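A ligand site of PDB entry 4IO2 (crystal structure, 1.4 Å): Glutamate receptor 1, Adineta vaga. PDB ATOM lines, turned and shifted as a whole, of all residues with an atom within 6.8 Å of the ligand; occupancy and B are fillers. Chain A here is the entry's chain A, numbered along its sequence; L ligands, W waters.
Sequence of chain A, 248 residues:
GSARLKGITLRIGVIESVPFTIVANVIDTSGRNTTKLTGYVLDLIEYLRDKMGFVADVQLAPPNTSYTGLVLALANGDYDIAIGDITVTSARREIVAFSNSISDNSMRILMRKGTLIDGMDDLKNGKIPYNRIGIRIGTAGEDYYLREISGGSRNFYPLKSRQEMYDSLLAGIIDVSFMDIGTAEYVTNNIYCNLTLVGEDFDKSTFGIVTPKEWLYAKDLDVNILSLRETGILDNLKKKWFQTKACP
Tyr 67 touches the ligand.
CA of Ile 86 touches O1 of the ligand (3.6 Å).
Thr 139 touches the ligand (CA to O4, 3.2 Å).
Arg 162 touches the ligand.
CA of Met 179 touches O3 of the ligand, at 3.8 Å.
Phe 207 touches the ligand.
12 residues have an atom within 4 Å of the ligand: Tyr 67, Asp 85, Ile 86, Thr 87, Arg 92, Arg 136, Thr 139, Ala 140, Arg 162, Met 179, Asp 180 and Phe 207.
Water W2 lies within hydrogen-bond range of an oxygen (O2) of the ligand (2.6 Å), the backbone NH (N) of Gly 141 (2.8 Å), the backbone NH (N) of Ala 140 (3.1 Å) and the side-chain sulfur (SD) of Met 107 (3.7 Å).
Water W3 lies within hydrogen-bond range of O3 of the ligand (2.7 Å), OG1 of Thr 183 (2.8 Å) and NE of Arg 162 (2.9 Å).
Water W1 lies within hydrogen-bond range of O2 of the ligand (2.7 Å), O of Phe 178 (3.2 Å), SD of Met 107 (3.3 Å), NH2 of Arg 136 (3.3 Å) and N of Met 179 (3.4 Å).
OD1 of Asp 85 sits at hydrogen-bond distance from OH of Tyr 67.
OD2 of Asp 85 is in salt-bridge range of NH2 of Arg 162.
The side-chain carboxylate of Asp 85 lies within hydrogen-bond range of the side-chain hydroxyl of Ser 17, 2.8 Å away.
The backbone carbonyl oxygen of Gly 138 sits at hydrogen-bond distance from the guanidinium group of Arg 92 (3.3 Å).
The side-chain hydroxyl of Thr 89 sits at hydrogen-bond distance from the backbone NH of Arg 92, 3.1 Å away.
O of Arg 136 lies within hydrogen-bond range of OG1 of Thr 139.
The guanidinium group (NE) of Arg 136 is in hydrogen-bond range of the side-chain sulfur (SD) of Met 165 (3.5 Å).
N of Gly 141 lies close to OG1 of Thr 139.
O3 of the ligand lies within hydrogen-bond range of N of Asp 180.
OD2 of Asp 180 is in salt-bridge range of N1 of the ligand (2.8 Å).
N1 of the ligand is in hydrogen-bond range of O of Asp 85.
The guanidinium group (NH1) of Arg 92 is in salt-bridge range of an oxygen (O1) of the ligand (2.8 Å).
O1 of the ligand is in hydrogen-bond range of N of Thr 87, at 2.9 Å.
The side-chain hydroxyl of Thr 87 sits at hydrogen-bond distance from a nitrogen (N1) of the ligand (2.8 Å).
An oxygen (O3) of the ligand lies within salt-bridge range of the guanidinium group (NH2) of Arg 136 (2.8 Å).
N of Ala 140 lies within hydrogen-bond range of O4 of the ligand (2.9 Å).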
ATOM      1  N   SER A  17      30.519  17.284 -13.414  1.00  0.00           N
ATOM      2  CA  SER A  17      30.361  18.228 -14.509  1.00  0.00           C
ATOM      3  C   SER A  17      29.704  19.477 -13.940  1.00  0.00           C
ATOM      4  O   SER A  17      28.503  19.464 -13.670  1.00  0.00           O
ATOM      5  CB  SER A  17      29.464  17.669 -15.599  1.00  0.00           C
ATOM      6  OG  SER A  17      29.421  18.588 -16.662  1.00  0.00           O
ATOM      7  N   TYR A  67      31.759   9.463 -20.431  1.00  0.00           N
ATOM      8  CA  TYR A  67      30.302   9.407 -20.534  1.00  0.00           C
ATOM      9  C   TYR A  67      29.886   8.042 -21.088  1.00  0.00           C
ATOM     10  O   TYR A  67      28.974   7.405 -20.520  1.00  0.00           O
ATOM     11  CB  TYR A  67      29.793  10.613 -21.351  1.00  0.00           C
ATOM     12  CG  TYR A  67      29.705  11.824 -20.458  1.00  0.00           C
ATOM     13  CD1 TYR A  67      30.835  12.573 -20.171  1.00  0.00           C
ATOM     14  CD2 TYR A  67      28.519  12.181 -19.870  1.00  0.00           C
ATOM     15  CE1 TYR A  67      30.786  13.668 -19.298  1.00  0.00           C
ATOM     16  CE2 TYR A  67      28.432  13.247 -18.967  1.00  0.00           C
ATOM     17  CZ  TYR A  67      29.582  13.987 -18.702  1.00  0.00           C
ATOM     18  OH  TYR A  67      29.559  15.075 -17.842  1.00  0.00           O
ATOM     19  N   THR A  68      30.516   7.578 -22.162  1.00  0.00           N
ATOM     20  CA  THR A  68      30.154   6.271 -22.644  1.00  0.00           C
ATOM     21  C   THR A  68      30.522   5.184 -21.628  1.00  0.00           C
ATOM     22  O   THR A  68      29.775   4.205 -21.494  1.00  0.00           O
ATOM     23  CB  THR A  68      30.664   6.025 -24.079  1.00  0.00           C
ATOM     24  OG1 THR A  68      29.956   6.911 -24.951  1.00  0.00           O
ATOM     25  CG2 THR A  68      30.327   4.575 -24.506  1.00  0.00           C
ATOM     26  N   VAL A  71      27.621   4.890 -19.169  1.00  0.00           N
ATOM     27  CA  VAL A  71      26.531   4.143 -19.777  1.00  0.00           C
ATOM     28  C   VAL A  71      26.839   2.638 -19.731  1.00  0.00           C
ATOM     29  O   VAL A  71      25.966   1.827 -19.372  1.00  0.00           O
ATOM     30  CB  VAL A  71      26.312   4.641 -21.216  1.00  0.00           C
ATOM     31  CG1 VAL A  71      25.377   3.771 -21.995  1.00  0.00           C
ATOM     32  CG2 VAL A  71      25.802   6.090 -21.175  1.00  0.00           C
ATOM     33  N   ASP A  85      24.369  15.143 -17.443  1.00  0.00           N
ATOM     34  CA  ASP A  85      24.398  15.736 -18.792  1.00  0.00           C
ATOM     35  C   ASP A  85      24.820  14.666 -19.788  1.00  0.00           C
ATOM     36  O   ASP A  85      25.898  14.745 -20.367  1.00  0.00           O
ATOM     37  CB  ASP A  85      25.332  16.963 -18.836  1.00  0.00           C
ATOM     38  CG  ASP A  85      26.727  16.753 -18.252  1.00  0.00           C
ATOM     39  OD1 ASP A  85      26.979  15.813 -17.487  1.00  0.00           O
ATOM     40  OD2 ASP A  85      27.620  17.602 -18.549  1.00  0.00           O
ATOM     41  N   ILE A  86      23.943  13.663 -19.951  1.00  0.00           N
ATOM     42  CA  ILE A  86      24.240  12.467 -20.722  1.00  0.00           C
ATOM     43  C   ILE A  86      23.399  12.489 -21.985  1.00  0.00           C
ATOM     44  O   ILE A  86      22.158  12.433 -21.943  1.00  0.00           O
ATOM     45  CB  ILE A  86      23.919  11.193 -19.916  1.00  0.00           C
ATOM     46  CG1 ILE A  86      24.647  11.179 -18.563  1.00  0.00           C
ATOM     47  CG2 ILE A  86      24.282   9.979 -20.686  1.00  0.00           C
ATOM     48  CD1 ILE A  86      24.068  10.171 -17.571  1.00  0.00           C
ATOM     49  N   THR A  87      24.071  12.642 -23.125  1.00  0.00           N
ATOM     50  CA  THR A  87      23.396  12.728 -24.395  1.00  0.00           C
ATOM     51  C   THR A  87      22.773  11.410 -24.837  1.00  0.00           C
ATOM     52  O   THR A  87      23.405  10.349 -24.806  1.00  0.00           O
ATOM     53  CB  THR A  87      24.354  13.246 -25.473  1.00  0.00           C
ATOM     54  OG1 THR A  87      24.927  14.488 -25.019  1.00  0.00           O
ATOM     55  CG2 THR A  87      23.662  13.476 -26.827  1.00  0.00           C
ATOM     56  N   VAL A  88      21.535  11.478 -25.315  1.00  0.00           N
ATOM     57  CA  VAL A  88      20.824  10.314 -25.871  1.00  0.00           C
ATOM     58  C   VAL A  88      21.349  10.116 -27.280  1.00  0.00           C
ATOM     59  O   VAL A  88      21.256  11.009 -28.140  1.00  0.00           O
ATOM     60  CB  VAL A  88      19.327  10.574 -25.883  1.00  0.00           C
ATOM     61  CG1 VAL A  88      18.608   9.344 -26.420  1.00  0.00           C
ATOM     62  CG2 VAL A  88      18.843  10.912 -24.449  1.00  0.00           C
ATOM     63  N   THR A  89      21.967   8.976 -27.543  1.00  0.00           N
ATOM     64  CA  THR A  89      22.504   8.675 -28.875  1.00  0.00           C
ATOM     65  C   THR A  89      22.028   7.311 -29.346  1.00  0.00           C
ATOM     66  O   THR A  89      21.683   6.463 -28.567  1.00  0.00           O
ATOM     67  CB  THR A  89      24.046   8.656 -28.948  1.00  0.00           C
ATOM     68  OG1 THR A  89      24.518   7.511 -28.254  1.00  0.00           O
ATOM     69  CG2 THR A  89      24.683   9.933 -28.326  1.00  0.00           C
ATOM     70  N   ARG A  92      24.182   4.490 -27.972  1.00  0.00           N
ATOM     71  CA  ARG A  92      23.890   4.169 -26.555  1.00  0.00           C
ATOM     72  C   ARG A  92      22.552   3.468 -26.383  1.00  0.00           C
ATOM     73  O   ARG A  92      22.408   2.596 -25.541  1.00  0.00           O
ATOM     74  CB  ARG A  92      23.975   5.434 -25.695  1.00  0.00           C
ATOM     75  CG  ARG A  92      25.392   5.953 -25.537  1.00  0.00           C
ATOM     76  CD  ARG A  92      25.445   7.380 -25.018  1.00  0.00           C
ATOM     77  NE  ARG A  92      26.803   7.879 -24.915  1.00  0.00           N
ATOM     78  CZ  ARG A  92      27.138   9.106 -24.529  1.00  0.00           C
ATOM     79  NH1 ARG A  92      26.189   9.950 -24.187  1.00  0.00           N
ATOM     80  NH2 ARG A  92      28.426   9.437 -24.450  1.00  0.00           N
ATOM     81  N   ASN A 105      19.632  19.954 -25.826  1.00  0.00           N
ATOM     82  CA  ASN A 105      21.079  20.109 -25.884  1.00  0.00           C
ATOM     83  C   ASN A 105      21.487  20.353 -27.304  1.00  0.00           C
ATOM     84  O   ASN A 105      20.755  20.038 -28.254  1.00  0.00           O
ATOM     85  CB  ASN A 105      21.791  18.835 -25.350  1.00  0.00           C
ATOM     86  CG  ASN A 105      23.297  19.002 -25.280  1.00  0.00           C
ATOM     87  OD1 ASN A 105      23.804  19.917 -24.649  1.00  0.00           O
ATOM     88  ND2 ASN A 105      24.030  18.098 -25.930  1.00  0.00           N
ATOM     89  N   MET A 107      25.728  21.269 -29.299  1.00  0.00           N
ATOM     90  CA  MET A 107      27.151  21.519 -29.056  1.00  0.00           C
ATOM     91  C   MET A 107      27.591  22.811 -29.689  1.00  0.00           C
ATOM     92  O   MET A 107      26.958  23.299 -30.628  1.00  0.00           O
ATOM     93  CB  MET A 107      28.061  20.370 -29.551  1.00  0.00           C
ATOM     94  CG  MET A 107      27.782  19.054 -28.867  1.00  0.00           C
ATOM     95  SD  MET A 107      29.010  17.790 -29.275  1.00  0.00           S
ATOM     96  CE  MET A 107      28.469  17.256 -30.870  1.00  0.00           C
ATOM     97  N   ARG A 136      37.233  14.974 -26.642  1.00  0.00           N
ATOM     98  CA  ARG A 136      37.152  14.088 -25.478  1.00  0.00           C
ATOM     99  C   ARG A 136      36.602  12.713 -25.842  1.00  0.00           C
ATOM    100  O   ARG A 136      35.467  12.559 -26.317  1.00  0.00           O
ATOM    101  CB  ARG A 136      36.316  14.730 -24.382  1.00  0.00           C
ATOM    102  CG  ARG A 136      36.971  15.930 -23.729  1.00  0.00           C
ATOM    103  CD  ARG A 136      35.992  16.680 -22.847  1.00  0.00           C
ATOM    104  NE  ARG A 136      35.022  17.405 -23.690  1.00  0.00           N
ATOM    105  CZ  ARG A 136      33.786  17.717 -23.370  1.00  0.00           C
ATOM    106  NH1 ARG A 136      33.270  17.290 -22.210  1.00  0.00           N
ATOM    107  NH2 ARG A 136      33.061  18.450 -24.195  1.00  0.00           N
ATOM    108  N   GLY A 138      34.910   9.208 -25.752  1.00  0.00           N
ATOM    109  CA  GLY A 138      33.737   8.681 -25.054  1.00  0.00           C
ATOM    110  C   GLY A 138      32.622   9.686 -24.866  1.00  0.00           C
ATOM    111  O   GLY A 138      31.709   9.467 -24.101  1.00  0.00           O
ATOM    112  N   THR A 139      32.706  10.802 -25.553  1.00  0.00           N
ATOM    113  CA  THR A 139      31.617  11.748 -25.616  1.00  0.00           C
ATOM    114  C   THR A 139      30.867  11.578 -26.959  1.00  0.00           C
ATOM    115  O   THR A 139      31.396  11.047 -27.945  1.00  0.00           O
ATOM    116  CB  THR A 139      32.061  13.228 -25.463  1.00  0.00           C
ATOM    117  OG1 THR A 139      32.918  13.593 -26.562  1.00  0.00           O
ATOM    118  CG2 THR A 139      32.790  13.469 -24.172  1.00  0.00           C
ATOM    119  N   ALA A 140      29.662  12.084 -26.989  1.00  0.00           N
ATOM    120  CA  ALA A 140      28.889  12.059 -28.210  1.00  0.00           C
ATOM    121  C   ALA A 140      29.602  12.863 -29.305  1.00  0.00           C
ATOM    122  O   ALA A 140      29.454  12.552 -30.474  1.00  0.00           O
ATOM    123  CB  ALA A 140      27.459  12.600 -27.936  1.00  0.00           C
ATOM    124  N   GLY A 141      30.365  13.873 -28.921  1.00  0.00           N
ATOM    125  CA  GLY A 141      31.125  14.682 -29.843  1.00  0.00           C
ATOM    126  C   GLY A 141      32.115  13.864 -30.667  1.00  0.00           C
ATOM    127  O   GLY A 141      32.437  14.206 -31.798  1.00  0.00           O
ATOM    128  N   ARG A 162      37.653  17.202 -19.338  1.00  0.00           N
ATOM    129  CA  ARG A 162      37.484  18.631 -19.544  1.00  0.00           C
ATOM    130  C   ARG A 162      38.751  19.419 -19.217  1.00  0.00           C
ATOM    131  O   ARG A 162      39.149  20.319 -19.945  1.00  0.00           O
ATOM    132  CB  ARG A 162      36.289  19.147 -18.750  1.00  0.00           C
ATOM    133  CG  ARG A 162      34.973  18.635 -19.292  1.00  0.00           C
ATOM    134  CD  ARG A 162      33.803  19.268 -18.554  1.00  0.00           C
ATOM    135  NE  ARG A 162      32.523  18.734 -19.017  1.00  0.00           N
ATOM    136  CZ  ARG A 162      31.897  17.658 -18.539  1.00  0.00           C
ATOM    137  NH1 ARG A 162      32.362  16.961 -17.520  1.00  0.00           N
ATOM    138  NH2 ARG A 162      30.770  17.294 -19.110  1.00  0.00           N
ATOM    139  N   MET A 165      41.050  19.378 -21.998  1.00  0.00           N
ATOM    140  CA  MET A 165      40.547  20.226 -23.054  1.00  0.00           C
ATOM    141  C   MET A 165      40.952  21.679 -22.764  1.00  0.00           C
ATOM    142  O   MET A 165      41.507  22.351 -23.626  1.00  0.00           O
ATOM    143  CB  MET A 165      39.039  20.062 -23.219  1.00  0.00           C
ATOM    144  CG  MET A 165      38.385  20.828 -24.321  1.00  0.00           C
ATOM    145  SD  MET A 165      36.648  20.403 -24.429  1.00  0.00           S
ATOM    146  CE  MET A 165      35.993  20.965 -22.839  1.00  0.00           C
ATOM    147  N   PHE A 178      34.908  20.605 -28.968  1.00  0.00           N
ATOM    148  CA  PHE A 178      33.451  20.668 -28.956  1.00  0.00           C
ATOM    149  C   PHE A 178      33.009  20.509 -27.512  1.00  0.00           C
ATOM    150  O   PHE A 178      33.642  19.774 -26.727  1.00  0.00           O
ATOM    151  CB  PHE A 178      32.838  19.475 -29.707  1.00  0.00           C
ATOM    152  CG  PHE A 178      33.169  19.366 -31.176  1.00  0.00           C
ATOM    153  CD1 PHE A 178      33.643  20.438 -31.895  1.00  0.00           C
ATOM    154  CD2 PHE A 178      32.980  18.151 -31.842  1.00  0.00           C
ATOM    155  CE1 PHE A 178      33.936  20.310 -33.229  1.00  0.00           C
ATOM    156  CE2 PHE A 178      33.242  18.029 -33.171  1.00  0.00           C
ATOM    157  CZ  PHE A 178      33.732  19.116 -33.868  1.00  0.00           C
ATOM    158  N   MET A 179      31.919  21.162 -27.159  1.00  0.00           N
ATOM    159  CA  MET A 179      31.377  21.085 -25.794  1.00  0.00           C
ATOM    160  C   MET A 179      29.891  21.363 -25.816  1.00  0.00           C
ATOM    161  O   MET A 179      29.417  22.180 -26.585  1.00  0.00           O
ATOM    162  CB  MET A 179      32.120  22.055 -24.900  1.00  0.00           C
ATOM    163  CG  MET A 179      31.767  21.918 -23.455  1.00  0.00           C
ATOM    164  SD  MET A 179      32.846  23.014 -22.435  1.00  0.00           S
ATOM    165  CE  MET A 179      32.256  22.557 -20.784  1.00  0.00           C
ATOM    166  N   ASP A 180      29.130  20.614 -25.039  1.00  0.00           N
ATOM    167  CA  ASP A 180      27.708  20.889 -24.873  1.00  0.00           C
ATOM    168  C   ASP A 180      27.475  22.343 -24.511  1.00  0.00           C
ATOM    169  O   ASP A 180      28.208  22.923 -23.720  1.00  0.00           O
ATOM    170  CB  ASP A 180      27.123  20.055 -23.764  1.00  0.00           C
ATOM    171  CG  ASP A 180      27.035  18.575 -24.059  1.00  0.00           C
ATOM    172  OD1 ASP A 180      27.009  18.168 -25.254  1.00  0.00           O
ATOM    173  OD2 ASP A 180      26.933  17.848 -23.038  1.00  0.00           O
ATOM    174  N   ILE A 181      26.397  22.913 -25.037  1.00  0.00           N
ATOM    175  CA  ILE A 181      26.194  24.342 -24.913  1.00  0.00           C
ATOM    176  C   ILE A 181      25.955  24.810 -23.479  1.00  0.00           C
ATOM    177  O   ILE A 181      26.442  25.882 -23.099  1.00  0.00           O
ATOM    178  CB  ILE A 181      25.018  24.813 -25.834  1.00  0.00           C
ATOM    179  CG1 ILE A 181      24.920  26.333 -25.889  1.00  0.00           C
ATOM    180  CG2 ILE A 181      23.667  24.165 -25.429  1.00  0.00           C
ATOM    181  CD1 ILE A 181      23.920  26.801 -26.961  1.00  0.00           C
ATOM    182  N   THR A 183      26.900  23.644 -20.350  1.00  0.00           N
ATOM    183  CA  THR A 183      28.139  23.698 -19.582  1.00  0.00           C
ATOM    184  C   THR A 183      29.218  24.584 -20.273  1.00  0.00           C
ATOM    185  O   THR A 183      30.030  25.211 -19.576  1.00  0.00           O
ATOM    186  CB  THR A 183      28.696  22.283 -19.290  1.00  0.00           C
ATOM    187  OG1 THR A 183      28.797  21.523 -20.525  1.00  0.00           O
ATOM    188  CG2 THR A 183      27.798  21.564 -18.260  1.00  0.00           C
ATOM    189  N   ALA A 184      29.245  24.643 -21.612  1.00  0.00           N
ATOM    190  CA  ALA A 184      30.223  25.484 -22.315  1.00  0.00           C
ATOM    191  C   ALA A 184      29.969  26.949 -21.955  1.00  0.00           C
ATOM    192  O   ALA A 184      30.904  27.695 -21.681  1.00  0.00           O
ATOM    193  CB  ALA A 184      30.088  25.296 -23.831  1.00  0.00           C
ATOM    194  N   PHE A 207      19.286  15.359 -23.341  1.00  0.00           N
ATOM    195  CA  PHE A 207      19.820  14.638 -22.203  1.00  0.00           C
ATOM    196  C   PHE A 207      18.680  13.796 -21.629  1.00  0.00           C
ATOM    197  O   PHE A 207      17.539  14.273 -21.524  1.00  0.00           O
ATOM    198  CB  PHE A 207      20.288  15.546 -21.094  1.00  0.00           C
ATOM    199  CG  PHE A 207      21.489  16.420 -21.439  1.00  0.00           C
ATOM    200  CD1 PHE A 207      22.455  16.043 -22.343  1.00  0.00           C
ATOM    201  CD2 PHE A 207      21.660  17.633 -20.785  1.00  0.00           C
ATOM    202  CE1 PHE A 207      23.547  16.855 -22.619  1.00  0.00           C
ATOM    203  CE2 PHE A 207      22.762  18.449 -21.044  1.00  0.00           C
ATOM    204  CZ  PHE A 207      23.699  18.063 -21.953  1.00  0.00           C
HETATM  205  N1  LIG L   1      26.817  15.098 -22.988  1.00  0.00           N
HETATM  206  C1  LIG L   1      28.066  14.499 -23.485  1.00  0.00           C
HETATM  207  C2  LIG L   1      27.907  12.984 -23.610  1.00  0.00           C
HETATM  208  O1  LIG L   1      26.918  12.429 -23.076  1.00  0.00           O
HETATM  209  C3  LIG L   1      29.259  14.799 -22.581  1.00  0.00           C
HETATM  210  C4  LIG L   1      29.567  16.282 -22.335  1.00  0.00           C
HETATM  211  C5  LIG L   1      30.114  17.047 -23.547  1.00  0.00           C
HETATM  212  O2  LIG L   1      30.391  16.419 -24.562  1.00  0.00           O
HETATM  213  O3  LIG L   1      30.329  18.284 -23.413  1.00  0.00           O
HETATM  214  O4  LIG L   1      28.754  12.348 -24.273  1.00  0.00           O
HETATM  215  O   HOH W   1      31.062  17.903 -26.747  1.00  0.00           O
HETATM  216  O   HOH W   2      29.334  15.191 -26.657  1.00  0.00           O
HETATM  217  O   HOH W   3      30.635  19.454 -21.034  1.00  0.00           O
